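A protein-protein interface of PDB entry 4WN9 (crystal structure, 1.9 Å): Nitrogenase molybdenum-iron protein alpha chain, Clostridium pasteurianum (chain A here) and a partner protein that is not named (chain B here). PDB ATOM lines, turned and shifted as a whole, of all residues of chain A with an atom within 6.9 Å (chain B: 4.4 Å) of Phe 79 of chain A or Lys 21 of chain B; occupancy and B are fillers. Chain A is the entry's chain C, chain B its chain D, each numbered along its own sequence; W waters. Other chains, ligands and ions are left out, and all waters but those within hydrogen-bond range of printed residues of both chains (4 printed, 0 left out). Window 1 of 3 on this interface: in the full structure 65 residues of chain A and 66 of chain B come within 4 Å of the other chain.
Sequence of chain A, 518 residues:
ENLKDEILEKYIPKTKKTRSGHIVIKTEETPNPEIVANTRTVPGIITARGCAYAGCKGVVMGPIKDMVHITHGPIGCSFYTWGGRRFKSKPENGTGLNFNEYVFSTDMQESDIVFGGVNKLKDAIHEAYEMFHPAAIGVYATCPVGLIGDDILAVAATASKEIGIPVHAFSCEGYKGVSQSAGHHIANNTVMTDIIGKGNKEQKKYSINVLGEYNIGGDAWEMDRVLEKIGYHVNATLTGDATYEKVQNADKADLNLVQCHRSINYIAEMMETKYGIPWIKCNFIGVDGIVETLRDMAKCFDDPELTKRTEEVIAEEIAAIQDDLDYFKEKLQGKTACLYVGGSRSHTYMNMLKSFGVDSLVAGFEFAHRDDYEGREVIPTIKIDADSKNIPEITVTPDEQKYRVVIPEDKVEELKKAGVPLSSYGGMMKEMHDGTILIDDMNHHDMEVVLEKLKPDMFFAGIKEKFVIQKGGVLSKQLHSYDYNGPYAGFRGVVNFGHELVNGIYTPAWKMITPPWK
Among the printed residues, pairs that only touch across the chains: Ile 75 of chain A with Pro 19 of chain B (3.7 Å), Ile 75 of chain A with Lys 21 of chain B (3.9 Å), Ile 75 of chain A with Thr 22 of chain B (3.6 Å), Gly 76 of chain A with Thr 22 of chain B (3.9 Å), Phe 79 of chain A with Lys 21 of chain B (3.7 Å), Phe 79 of chain A with Thr 22 of chain B (3.4 Å), Phe 79 of chain A with Tyr 394 of chain B (3.8 Å), Phe 79 of chain A with Pro 412 of chain B (3.9 Å), Trp 82 of chain A with Pro 19 of chain B (3.6 Å), Val 103 of chain A with Pro 19 of chain B (3.8 Å) and Gln 109 of chain A with Lys 21 of chain B (3.97 Å).
O of Trp 82 of chain A lies within hydrogen-bond range of OH of Tyr 394 of chain B, 2.7 Å away. The side-chain hydroxyl (OH) of Tyr 80 of chain A sits close to the side-chain hydroxyl (OG1) of Thr 22 of chain B (3.3 Å). The side-chain carboxylate of Asp 107 of chain A lies within salt-bridge range of the side-chain amino group of Lys 21 of chain B (2.9 Å).
Water W4 lies within hydrogen-bond range of OD2 of Asp 107 of chain A (2.7 Å) and NZ of Lys 21 of chain B (3.4 Å). Water W1 lies within hydrogen-bond range of the side-chain amide oxygen of Gln 109 of chain A and the backbone NH of Gly 144 of chain B. Water W3 lies within hydrogen-bond range of OH of Tyr 394 of chain B (2.8 Å) and O of Phe 79 of chain A (2.9 Å). Water W2 lies within hydrogen-bond range of the side-chain amide oxygen (OE1) of Gln 109 of chain A, the backbone carbonyl oxygen (O) of Gly 144 of chain B and the side-chain amino group (NZ) of Lys 21 of chain B.
O of Thr 22 of chain B lies within hydrogen-bond range of N of His 146 of chain B (2.8 Å). The backbone carbonyl oxygen (O) of Asp 107 of chain A is in hydrogen-bond range of the side-chain amide nitrogen (NE2) of Gln 109 of chain A, 2.9 Å away. N of Asp 107 of chain A is in hydrogen-bond range of OG of Ser 105 of chain A, at 2.9 Å.
Of the 11 printed residues of chain B, 5 touch a printed residue of chain A. Of the 18 printed residues of chain A, 8 touch a printed residue of chain B. Printed residues of chain A that touch a printed residue of chain B: Ile 75, Gly 76, Phe 79, Tyr 80, Trp 82, Val 103, Asp 107 and Gln 109. Hydrophobic or aromatic side chains of chain A that line the printed part of chain B: Ile 75, Phe 79, Tyr 80, Trp 82 and Val 103. Among the printed residues, Asp or Glu carboxylates within 4 Å of a Lys or Arg side-chain nitrogen of the other chain: Asp 107 of chain A with Lys 21 of chain B.
Of the printed residues of chain A, Thr 22 of chain B touches Ile 75 (3.6 Å), Gly 76 (3.9 Å), Phe 79 (3.4 Å) and Tyr 80 (3.2 Å). Of the printed residues of chain B, Tyr 80 of chain A touches Thr 22. Printed residues of chain B within 4 Å of Ile 75 of chain A: Pro 19 (3.7 Å), Lys 21 (3.9 Å) and Thr 22 (3.6 Å). Gly 144 of chain B touches none of the printed residues of chain A. The nearest residue of chain A that does not touch Lys 21 of chain B is Met 108 of chain A (5.9 Å). The nearest printed residue of chain A that does not touch Tyr 394 of chain B is Gly 83 of chain A (4.9 Å).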
ATOM      1  N   TYR A  53       4.104 -40.802 -11.343  1.00  0.00           N
ATOM      2  CA  TYR A  53       4.714 -39.461 -11.282  1.00  0.00           C
ATOM      3  C   TYR A  53       5.568 -39.306 -10.016  1.00  0.00           C
ATOM      4  O   TYR A  53       6.665 -38.754 -10.062  1.00  0.00           O
ATOM      5  CB  TYR A  53       3.641 -38.367 -11.355  1.00  0.00           C
ATOM      6  CG  TYR A  53       4.101 -37.028 -10.821  1.00  0.00           C
ATOM      7  CD1 TYR A  53       4.800 -36.136 -11.620  1.00  0.00           C
ATOM      8  CD2 TYR A  53       3.858 -36.672  -9.501  1.00  0.00           C
ATOM      9  CE1 TYR A  53       5.224 -34.908 -11.119  1.00  0.00           C
ATOM     10  CE2 TYR A  53       4.284 -35.449  -8.985  1.00  0.00           C
ATOM     11  CZ  TYR A  53       4.958 -34.572  -9.798  1.00  0.00           C
ATOM     12  OH  TYR A  53       5.392 -33.376  -9.274  1.00  0.00           O
ATOM     13  N   THR A  71       7.084 -29.617 -12.887  1.00  0.00           N
ATOM     14  CA  THR A  71       5.891 -30.409 -13.073  1.00  0.00           C
ATOM     15  C   THR A  71       4.965 -29.779 -14.078  1.00  0.00           C
ATOM     16  O   THR A  71       4.537 -28.642 -13.918  1.00  0.00           O
ATOM     17  CB  THR A  71       5.096 -30.574 -11.778  1.00  0.00           C
ATOM     18  OG1 THR A  71       5.921 -31.194 -10.807  1.00  0.00           O
ATOM     19  CG2 THR A  71       3.878 -31.444 -12.009  1.00  0.00           C
ATOM     20  N   PRO A  74      -1.555 -29.638 -13.211  1.00  0.00           N
ATOM     21  CA  PRO A  74      -2.148 -28.748 -12.233  1.00  0.00           C
ATOM     22  C   PRO A  74      -1.301 -28.760 -10.940  1.00  0.00           C
ATOM     23  O   PRO A  74      -0.280 -29.425 -10.880  1.00  0.00           O
ATOM     24  CB  PRO A  74      -3.557 -29.304 -12.045  1.00  0.00           C
ATOM     25  CG  PRO A  74      -3.648 -30.557 -12.878  1.00  0.00           C
ATOM     26  CD  PRO A  74      -2.285 -30.909 -13.346  1.00  0.00           C
ATOM     27  N   ILE A  75      -1.690 -27.989  -9.934  1.00  0.00           N
ATOM     28  CA  ILE A  75      -0.729 -27.591  -8.904  1.00  0.00           C
ATOM     29  C   ILE A  75      -0.408 -28.682  -7.851  1.00  0.00           C
ATOM     30  O   ILE A  75       0.678 -28.697  -7.278  1.00  0.00           O
ATOM     31  CB  ILE A  75      -1.202 -26.286  -8.231  1.00  0.00           C
ATOM     32  CG1 ILE A  75      -0.045 -25.569  -7.536  1.00  0.00           C
ATOM     33  CG2 ILE A  75      -2.364 -26.559  -7.287  1.00  0.00           C
ATOM     34  CD1 ILE A  75       1.107 -25.181  -8.446  1.00  0.00           C
ATOM     35  N   GLY A  76      -1.353 -29.573  -7.599  1.00  0.00           N
ATOM     36  CA  GLY A  76      -1.193 -30.611  -6.571  1.00  0.00           C
ATOM     37  C   GLY A  76       0.029 -31.489  -6.752  1.00  0.00           C
ATOM     38  O   GLY A  76       0.827 -31.636  -5.840  1.00  0.00           O
ATOM     39  N   CYS A  77       0.168 -32.086  -7.931  1.00  0.00           N
ATOM     40  CA  CYS A  77       1.327 -32.927  -8.215  1.00  0.00           C
ATOM     41  C   CYS A  77       2.596 -32.248  -7.762  1.00  0.00           C
ATOM     42  O   CYS A  77       3.496 -32.889  -7.201  1.00  0.00           O
ATOM     43  CB  CYS A  77       1.395 -33.238  -9.708  1.00  0.00           C
ATOM     44  SG  CYS A  77      -0.192 -33.738 -10.399  1.00  0.00           S
ATOM     45  N   SER A  78       2.693 -30.948  -8.029  1.00  0.00           N
ATOM     46  CA  SER A  78       3.829 -30.152  -7.585  1.00  0.00           C
ATOM     47  C   SER A  78       3.872 -29.923  -6.055  1.00  0.00           C
ATOM     48  O   SER A  78       4.864 -30.274  -5.403  1.00  0.00           O
ATOM     49  CB  SER A  78       3.805 -28.796  -8.307  1.00  0.00           C
ATOM     50  OG  SER A  78       4.901 -27.991  -7.921  1.00  0.00           O
ATOM     51  N   PHE A  79       2.806 -29.345  -5.489  1.00  0.00           N
ATOM     52  CA  PHE A  79       2.750 -28.995  -4.063  1.00  0.00           C
ATOM     53  C   PHE A  79       3.007 -30.215  -3.172  1.00  0.00           C
ATOM     54  O   PHE A  79       3.671 -30.125  -2.145  1.00  0.00           O
ATOM     55  CB  PHE A  79       1.380 -28.401  -3.727  1.00  0.00           C
ATOM     56  CG  PHE A  79       1.153 -28.124  -2.263  1.00  0.00           C
ATOM     57  CD1 PHE A  79       1.476 -26.885  -1.716  1.00  0.00           C
ATOM     58  CD2 PHE A  79       0.546 -29.080  -1.433  1.00  0.00           C
ATOM     59  CE1 PHE A  79       1.225 -26.610  -0.370  1.00  0.00           C
ATOM     60  CE2 PHE A  79       0.295 -28.798  -0.094  1.00  0.00           C
ATOM     61  CZ  PHE A  79       0.629 -27.573   0.433  1.00  0.00           C
ATOM     62  N   TYR A  80       2.504 -31.360  -3.583  1.00  0.00           N
ATOM     63  CA  TYR A  80       2.683 -32.529  -2.760  1.00  0.00           C
ATOM     64  C   TYR A  80       4.083 -33.141  -2.880  1.00  0.00           C
ATOM     65  O   TYR A  80       4.375 -34.138  -2.227  1.00  0.00           O
ATOM     66  CB  TYR A  80       1.566 -33.534  -3.023  1.00  0.00           C
ATOM     67  CG  TYR A  80       0.218 -33.007  -2.587  1.00  0.00           C
ATOM     68  CD1 TYR A  80      -0.035 -32.731  -1.247  1.00  0.00           C
ATOM     69  CD2 TYR A  80      -0.788 -32.764  -3.504  1.00  0.00           C
ATOM     70  CE1 TYR A  80      -1.249 -32.228  -0.836  1.00  0.00           C
ATOM     71  CE2 TYR A  80      -2.003 -32.247  -3.102  1.00  0.00           C
ATOM     72  CZ  TYR A  80      -2.233 -31.985  -1.768  1.00  0.00           C
ATOM     73  OH  TYR A  80      -3.451 -31.494  -1.357  1.00  0.00           O
ATOM     74  N   THR A  81       4.971 -32.523  -3.655  1.00  0.00           N
ATOM     75  CA  THR A  81       6.385 -32.942  -3.662  1.00  0.00           C
ATOM     76  C   THR A  81       7.243 -31.853  -3.057  1.00  0.00           C
ATOM     77  O   THR A  81       8.458 -31.840  -3.223  1.00  0.00           O
ATOM     78  CB  THR A  81       6.889 -33.353  -5.072  1.00  0.00           C
ATOM     79  OG1 THR A  81       6.714 -32.268  -5.991  1.00  0.00           O
ATOM     80  CG2 THR A  81       6.104 -34.576  -5.597  1.00  0.00           C
ATOM     81  N   TRP A  82       6.613 -30.941  -2.321  1.00  0.00           N
ATOM     82  CA  TRP A  82       7.355 -29.839  -1.700  1.00  0.00           C
ATOM     83  C   TRP A  82       7.813 -30.175  -0.282  1.00  0.00           C
ATOM     84  O   TRP A  82       7.155 -29.784   0.686  1.00  0.00           O
ATOM     85  CB  TRP A  82       6.486 -28.598  -1.703  1.00  0.00           C
ATOM     86  CG  TRP A  82       7.182 -27.319  -1.413  1.00  0.00           C
ATOM     87  CD1 TRP A  82       8.514 -27.115  -1.232  1.00  0.00           C
ATOM     88  CD2 TRP A  82       6.559 -26.037  -1.305  1.00  0.00           C
ATOM     89  NE1 TRP A  82       8.759 -25.774  -0.997  1.00  0.00           N
ATOM     90  CE2 TRP A  82       7.570 -25.097  -1.043  1.00  0.00           C
ATOM     91  CE3 TRP A  82       5.239 -25.597  -1.391  1.00  0.00           C
ATOM     92  CZ2 TRP A  82       7.293 -23.744  -0.856  1.00  0.00           C
ATOM     93  CZ3 TRP A  82       4.965 -24.249  -1.194  1.00  0.00           C
ATOM     94  CH2 TRP A  82       5.979 -23.347  -0.944  1.00  0.00           C
ATOM     95  N   GLY A  83       8.922 -30.924  -0.180  1.00  0.00           N
ATOM     96  CA  GLY A  83       9.621 -31.158   1.090  1.00  0.00           C
ATOM     97  C   GLY A  83       9.200 -32.373   1.922  1.00  0.00           C
ATOM     98  O   GLY A  83       9.817 -32.693   2.949  1.00  0.00           O
ATOM     99  N   GLY A  84       8.174 -33.074   1.489  1.00  0.00           N
ATOM    100  CA  GLY A  84       7.706 -34.246   2.243  1.00  0.00           C
ATOM    101  C   GLY A  84       8.664 -35.425   2.256  1.00  0.00           C
ATOM    102  O   GLY A  84       8.703 -36.190   3.219  1.00  0.00           O
ATOM    103  N   VAL A 103       9.495 -25.836  -5.351  1.00  0.00           N
ATOM    104  CA  VAL A 103       8.829 -26.663  -6.333  1.00  0.00           C
ATOM    105  C   VAL A 103       8.411 -25.766  -7.502  1.00  0.00           C
ATOM    106  O   VAL A 103       8.123 -24.574  -7.320  1.00  0.00           O
ATOM    107  CB  VAL A 103       7.638 -27.461  -5.766  1.00  0.00           C
ATOM    108  CG1 VAL A 103       8.154 -28.621  -4.899  1.00  0.00           C
ATOM    109  CG2 VAL A 103       6.672 -26.569  -4.993  1.00  0.00           C
ATOM    110  N   SER A 105       6.218 -25.575 -11.355  1.00  0.00           N
ATOM    111  CA  SER A 105       4.986 -26.054 -11.922  1.00  0.00           C
ATOM    112  C   SER A 105       4.545 -25.208 -13.114  1.00  0.00           C
ATOM    113  O   SER A 105       4.892 -24.033 -13.221  1.00  0.00           O
ATOM    114  CB  SER A 105       3.912 -25.911 -10.853  1.00  0.00           C
ATOM    115  OG  SER A 105       2.692 -26.437 -11.276  1.00  0.00           O
ATOM    116  N   ASP A 107       1.301 -25.220 -13.448  1.00  0.00           N
ATOM    117  CA  ASP A 107       0.055 -24.804 -12.824  1.00  0.00           C
ATOM    118  C   ASP A 107      -1.045 -24.734 -13.877  1.00  0.00           C
ATOM    119  O   ASP A 107      -1.674 -23.683 -14.078  1.00  0.00           O
ATOM    120  CB  ASP A 107       0.284 -23.440 -12.158  1.00  0.00           C
ATOM    121  CG  ASP A 107      -0.905 -22.940 -11.371  1.00  0.00           C
ATOM    122  OD1 ASP A 107      -1.883 -23.704 -11.139  1.00  0.00           O
ATOM    123  OD2 ASP A 107      -0.855 -21.745 -10.983  1.00  0.00           O
ATOM    124  N   MET A 108      -1.294 -25.870 -14.529  1.00  0.00           N
ATOM    125  CA  MET A 108      -2.242 -25.913 -15.629  1.00  0.00           C
ATOM    126  C   MET A 108      -3.606 -25.469 -15.162  1.00  0.00           C
ATOM    127  O   MET A 108      -4.037 -25.792 -14.060  1.00  0.00           O
ATOM    128  CB  MET A 108      -2.345 -27.315 -16.233  1.00  0.00           C
ATOM    129  CG  MET A 108      -1.118 -27.736 -17.015  1.00  0.00           C
ATOM    130  SD  MET A 108      -1.104 -29.490 -17.474  1.00  0.00           S
ATOM    131  CE  MET A 108      -2.032 -29.484 -19.002  1.00  0.00           C
ATOM    132  N   GLN A 109      -4.266 -24.716 -16.032  1.00  0.00           N
ATOM    133  CA  GLN A 109      -5.624 -24.275 -15.848  1.00  0.00           C
ATOM    134  C   GLN A 109      -6.502 -24.941 -16.906  1.00  0.00           C
ATOM    135  O   GLN A 109      -6.005 -25.607 -17.814  1.00  0.00           O
ATOM    136  CB  GLN A 109      -5.697 -22.758 -16.044  1.00  0.00           C
ATOM    137  CG  GLN A 109      -4.695 -21.965 -15.217  1.00  0.00           C
ATOM    138  CD  GLN A 109      -5.011 -22.041 -13.744  1.00  0.00           C
ATOM    139  OE1 GLN A 109      -6.144 -21.806 -13.341  1.00  0.00           O
ATOM    140  NE2 GLN A 109      -4.014 -22.376 -12.932  1.00  0.00           N
ATOM    141  N   PRO B  19       3.785 -22.506  -4.432  1.00  0.00           N
ATOM    142  CA  PRO B  19       2.395 -22.075  -4.521  1.00  0.00           C
ATOM    143  C   PRO B  19       1.737 -21.775  -3.172  1.00  0.00           C
ATOM    144  O   PRO B  19       2.072 -22.392  -2.140  1.00  0.00           O
ATOM    145  CB  PRO B  19       1.692 -23.263  -5.175  1.00  0.00           C
ATOM    146  CG  PRO B  19       2.579 -24.436  -4.932  1.00  0.00           C
ATOM    147  CD  PRO B  19       3.973 -23.892  -4.897  1.00  0.00           C
ATOM    148  N   ALA B  20       0.801 -20.832  -3.208  1.00  0.00           N
ATOM    149  CA  ALA B  20       0.029 -20.450  -2.044  1.00  0.00           C
ATOM    150  C   ALA B  20      -1.355 -21.047  -2.160  1.00  0.00           C
ATOM    151  O   ALA B  20      -2.364 -20.406  -1.872  1.00  0.00           O
ATOM    152  CB  ALA B  20      -0.045 -18.928  -1.932  1.00  0.00           C
ATOM    153  N   LYS B  21      -1.384 -22.290  -2.618  1.00  0.00           N
ATOM    154  CA  LYS B  21      -2.596 -23.063  -2.758  1.00  0.00           C
ATOM    155  C   LYS B  21      -2.199 -24.498  -3.051  1.00  0.00           C
ATOM    156  O   LYS B  21      -1.054 -24.779  -3.359  1.00  0.00           O
ATOM    157  CB  LYS B  21      -3.444 -22.582  -3.936  1.00  0.00           C
ATOM    158  CG  LYS B  21      -2.689 -22.581  -5.252  1.00  0.00           C
ATOM    159  CD  LYS B  21      -3.608 -22.638  -6.470  1.00  0.00           C
ATOM    160  CE  LYS B  21      -2.786 -22.741  -7.754  1.00  0.00           C
ATOM    161  NZ  LYS B  21      -3.609 -22.778  -9.000  1.00  0.00           N
ATOM    162  N   THR B  22      -3.173 -25.383  -2.976  1.00  0.00           N
ATOM    163  CA  THR B  22      -3.055 -26.701  -3.526  1.00  0.00           C
ATOM    164  C   THR B  22      -4.365 -27.013  -4.278  1.00  0.00           C
ATOM    165  O   THR B  22      -5.215 -26.116  -4.454  1.00  0.00           O
ATOM    166  CB  THR B  22      -2.646 -27.783  -2.477  1.00  0.00           C
ATOM    167  OG1 THR B  22      -2.371 -29.020  -3.168  1.00  0.00           O
ATOM    168  CG2 THR B  22      -3.732 -28.023  -1.455  1.00  0.00           C
ATOM    169  N   GLY B 144      -9.282 -23.402  -9.953  1.00  0.00           N
ATOM    170  CA  GLY B 144      -9.260 -22.853  -8.622  1.00  0.00           C
ATOM    171  C   GLY B 144      -8.252 -23.564  -7.743  1.00  0.00           C
ATOM    172  O   GLY B 144      -7.096 -23.762  -8.139  1.00  0.00           O
ATOM    173  N   SER B 145      -8.696 -23.951  -6.554  1.00  0.00           N
ATOM    174  CA  SER B 145      -7.781 -24.450  -5.523  1.00  0.00           C
ATOM    175  C   SER B 145      -8.517 -25.392  -4.593  1.00  0.00           C
ATOM    176  O   SER B 145      -9.696 -25.668  -4.783  1.00  0.00           O
ATOM    177  CB  SER B 145      -7.225 -23.288  -4.708  1.00  0.00           C
ATOM    178  OG  SER B 145      -8.166 -22.814  -3.752  1.00  0.00           O
ATOM    179  N   HIS B 146      -7.827 -25.857  -3.555  1.00  0.00           N
ATOM    180  CA  HIS B 146      -8.459 -26.712  -2.569  1.00  0.00           C
ATOM    181  C   HIS B 146      -9.704 -26.088  -1.946  1.00  0.00           C
ATOM    182  O   HIS B 146     -10.635 -26.813  -1.585  1.00  0.00           O
ATOM    183  CB  HIS B 146      -7.448 -27.068  -1.476  1.00  0.00           C
ATOM    184  CG  HIS B 146      -6.868 -25.873  -0.789  1.00  0.00           C
ATOM    185  ND1 HIS B 146      -5.936 -25.054  -1.385  1.00  0.00           N
ATOM    186  CD2 HIS B 146      -7.097 -25.354   0.439  1.00  0.00           C
ATOM    187  CE1 HIS B 146      -5.603 -24.084  -0.548  1.00  0.00           C
ATOM    188  NE2 HIS B 146      -6.304 -24.240   0.562  1.00  0.00           N
ATOM    189  N   GLY B 344      -3.233 -17.855  -3.280  1.00  0.00           N
ATOM    190  CA  GLY B 344      -2.976 -18.646  -4.462  1.00  0.00           C
ATOM    191  C   GLY B 344      -4.260 -18.967  -5.189  1.00  0.00           C
ATOM    192  O   GLY B 344      -4.243 -19.404  -6.345  1.00  0.00           O
ATOM    193  N   THR B 345      -5.366 -18.745  -4.498  1.00  0.00           N
ATOM    194  CA  THR B 345      -6.681 -19.069  -4.982  1.00  0.00           C
ATOM    195  C   THR B 345      -7.209 -17.958  -5.904  1.00  0.00           C
ATOM    196  O   THR B 345      -7.325 -16.795  -5.493  1.00  0.00           O
ATOM    197  CB  THR B 345      -7.662 -19.250  -3.821  1.00  0.00           C
ATOM    198  OG1 THR B 345      -7.319 -20.413  -3.019  1.00  0.00           O
ATOM    199  CG2 THR B 345      -9.061 -19.408  -4.356  1.00  0.00           C
ATOM    200  N   TYR B 394       4.949 -23.282   4.989  1.00  0.00           N
ATOM    201  CA  TYR B 394       5.953 -23.006   3.976  1.00  0.00           C
ATOM    202  C   TYR B 394       6.564 -21.635   4.082  1.00  0.00           C
ATOM    203  O   TYR B 394       7.552 -21.349   3.421  1.00  0.00           O
ATOM    204  CB  TYR B 394       5.374 -23.261   2.579  1.00  0.00           C
ATOM    205  CG  TYR B 394       5.257 -24.745   2.324  1.00  0.00           C
ATOM    206  CD1 TYR B 394       6.382 -25.509   2.024  1.00  0.00           C
ATOM    207  CD2 TYR B 394       4.052 -25.393   2.466  1.00  0.00           C
ATOM    208  CE1 TYR B 394       6.278 -26.887   1.817  1.00  0.00           C
ATOM    209  CE2 TYR B 394       3.939 -26.754   2.253  1.00  0.00           C
ATOM    210  CZ  TYR B 394       5.043 -27.497   1.937  1.00  0.00           C
ATOM    211  OH  TYR B 394       4.882 -28.856   1.718  1.00  0.00           O
ATOM    212  N   PRO B 412      -1.544 -25.776   5.022  1.00  0.00           N
ATOM    213  CA  PRO B 412      -1.386 -26.675   6.162  1.00  0.00           C
ATOM    214  C   PRO B 412      -0.249 -26.244   7.065  1.00  0.00           C
ATOM    215  O   PRO B 412       0.682 -25.599   6.597  1.00  0.00           O
ATOM    216  CB  PRO B 412      -1.007 -27.996   5.523  1.00  0.00           C
ATOM    217  CG  PRO B 412      -0.479 -27.670   4.173  1.00  0.00           C
ATOM    218  CD  PRO B 412      -0.793 -26.239   3.850  1.00  0.00           C
HETATM  219  O   HOH W   1      -8.446 -21.440 -11.994  1.00  0.00           O
HETATM  220  O   HOH W   2      -6.114 -23.226 -10.880  1.00  0.00           O
HETATM  221  O   HOH W   3       3.402 -30.896   0.594  1.00  0.00           O
HETATM  222  O   HOH W   4      -2.569 -19.833 -10.230  1.00  0.00           O
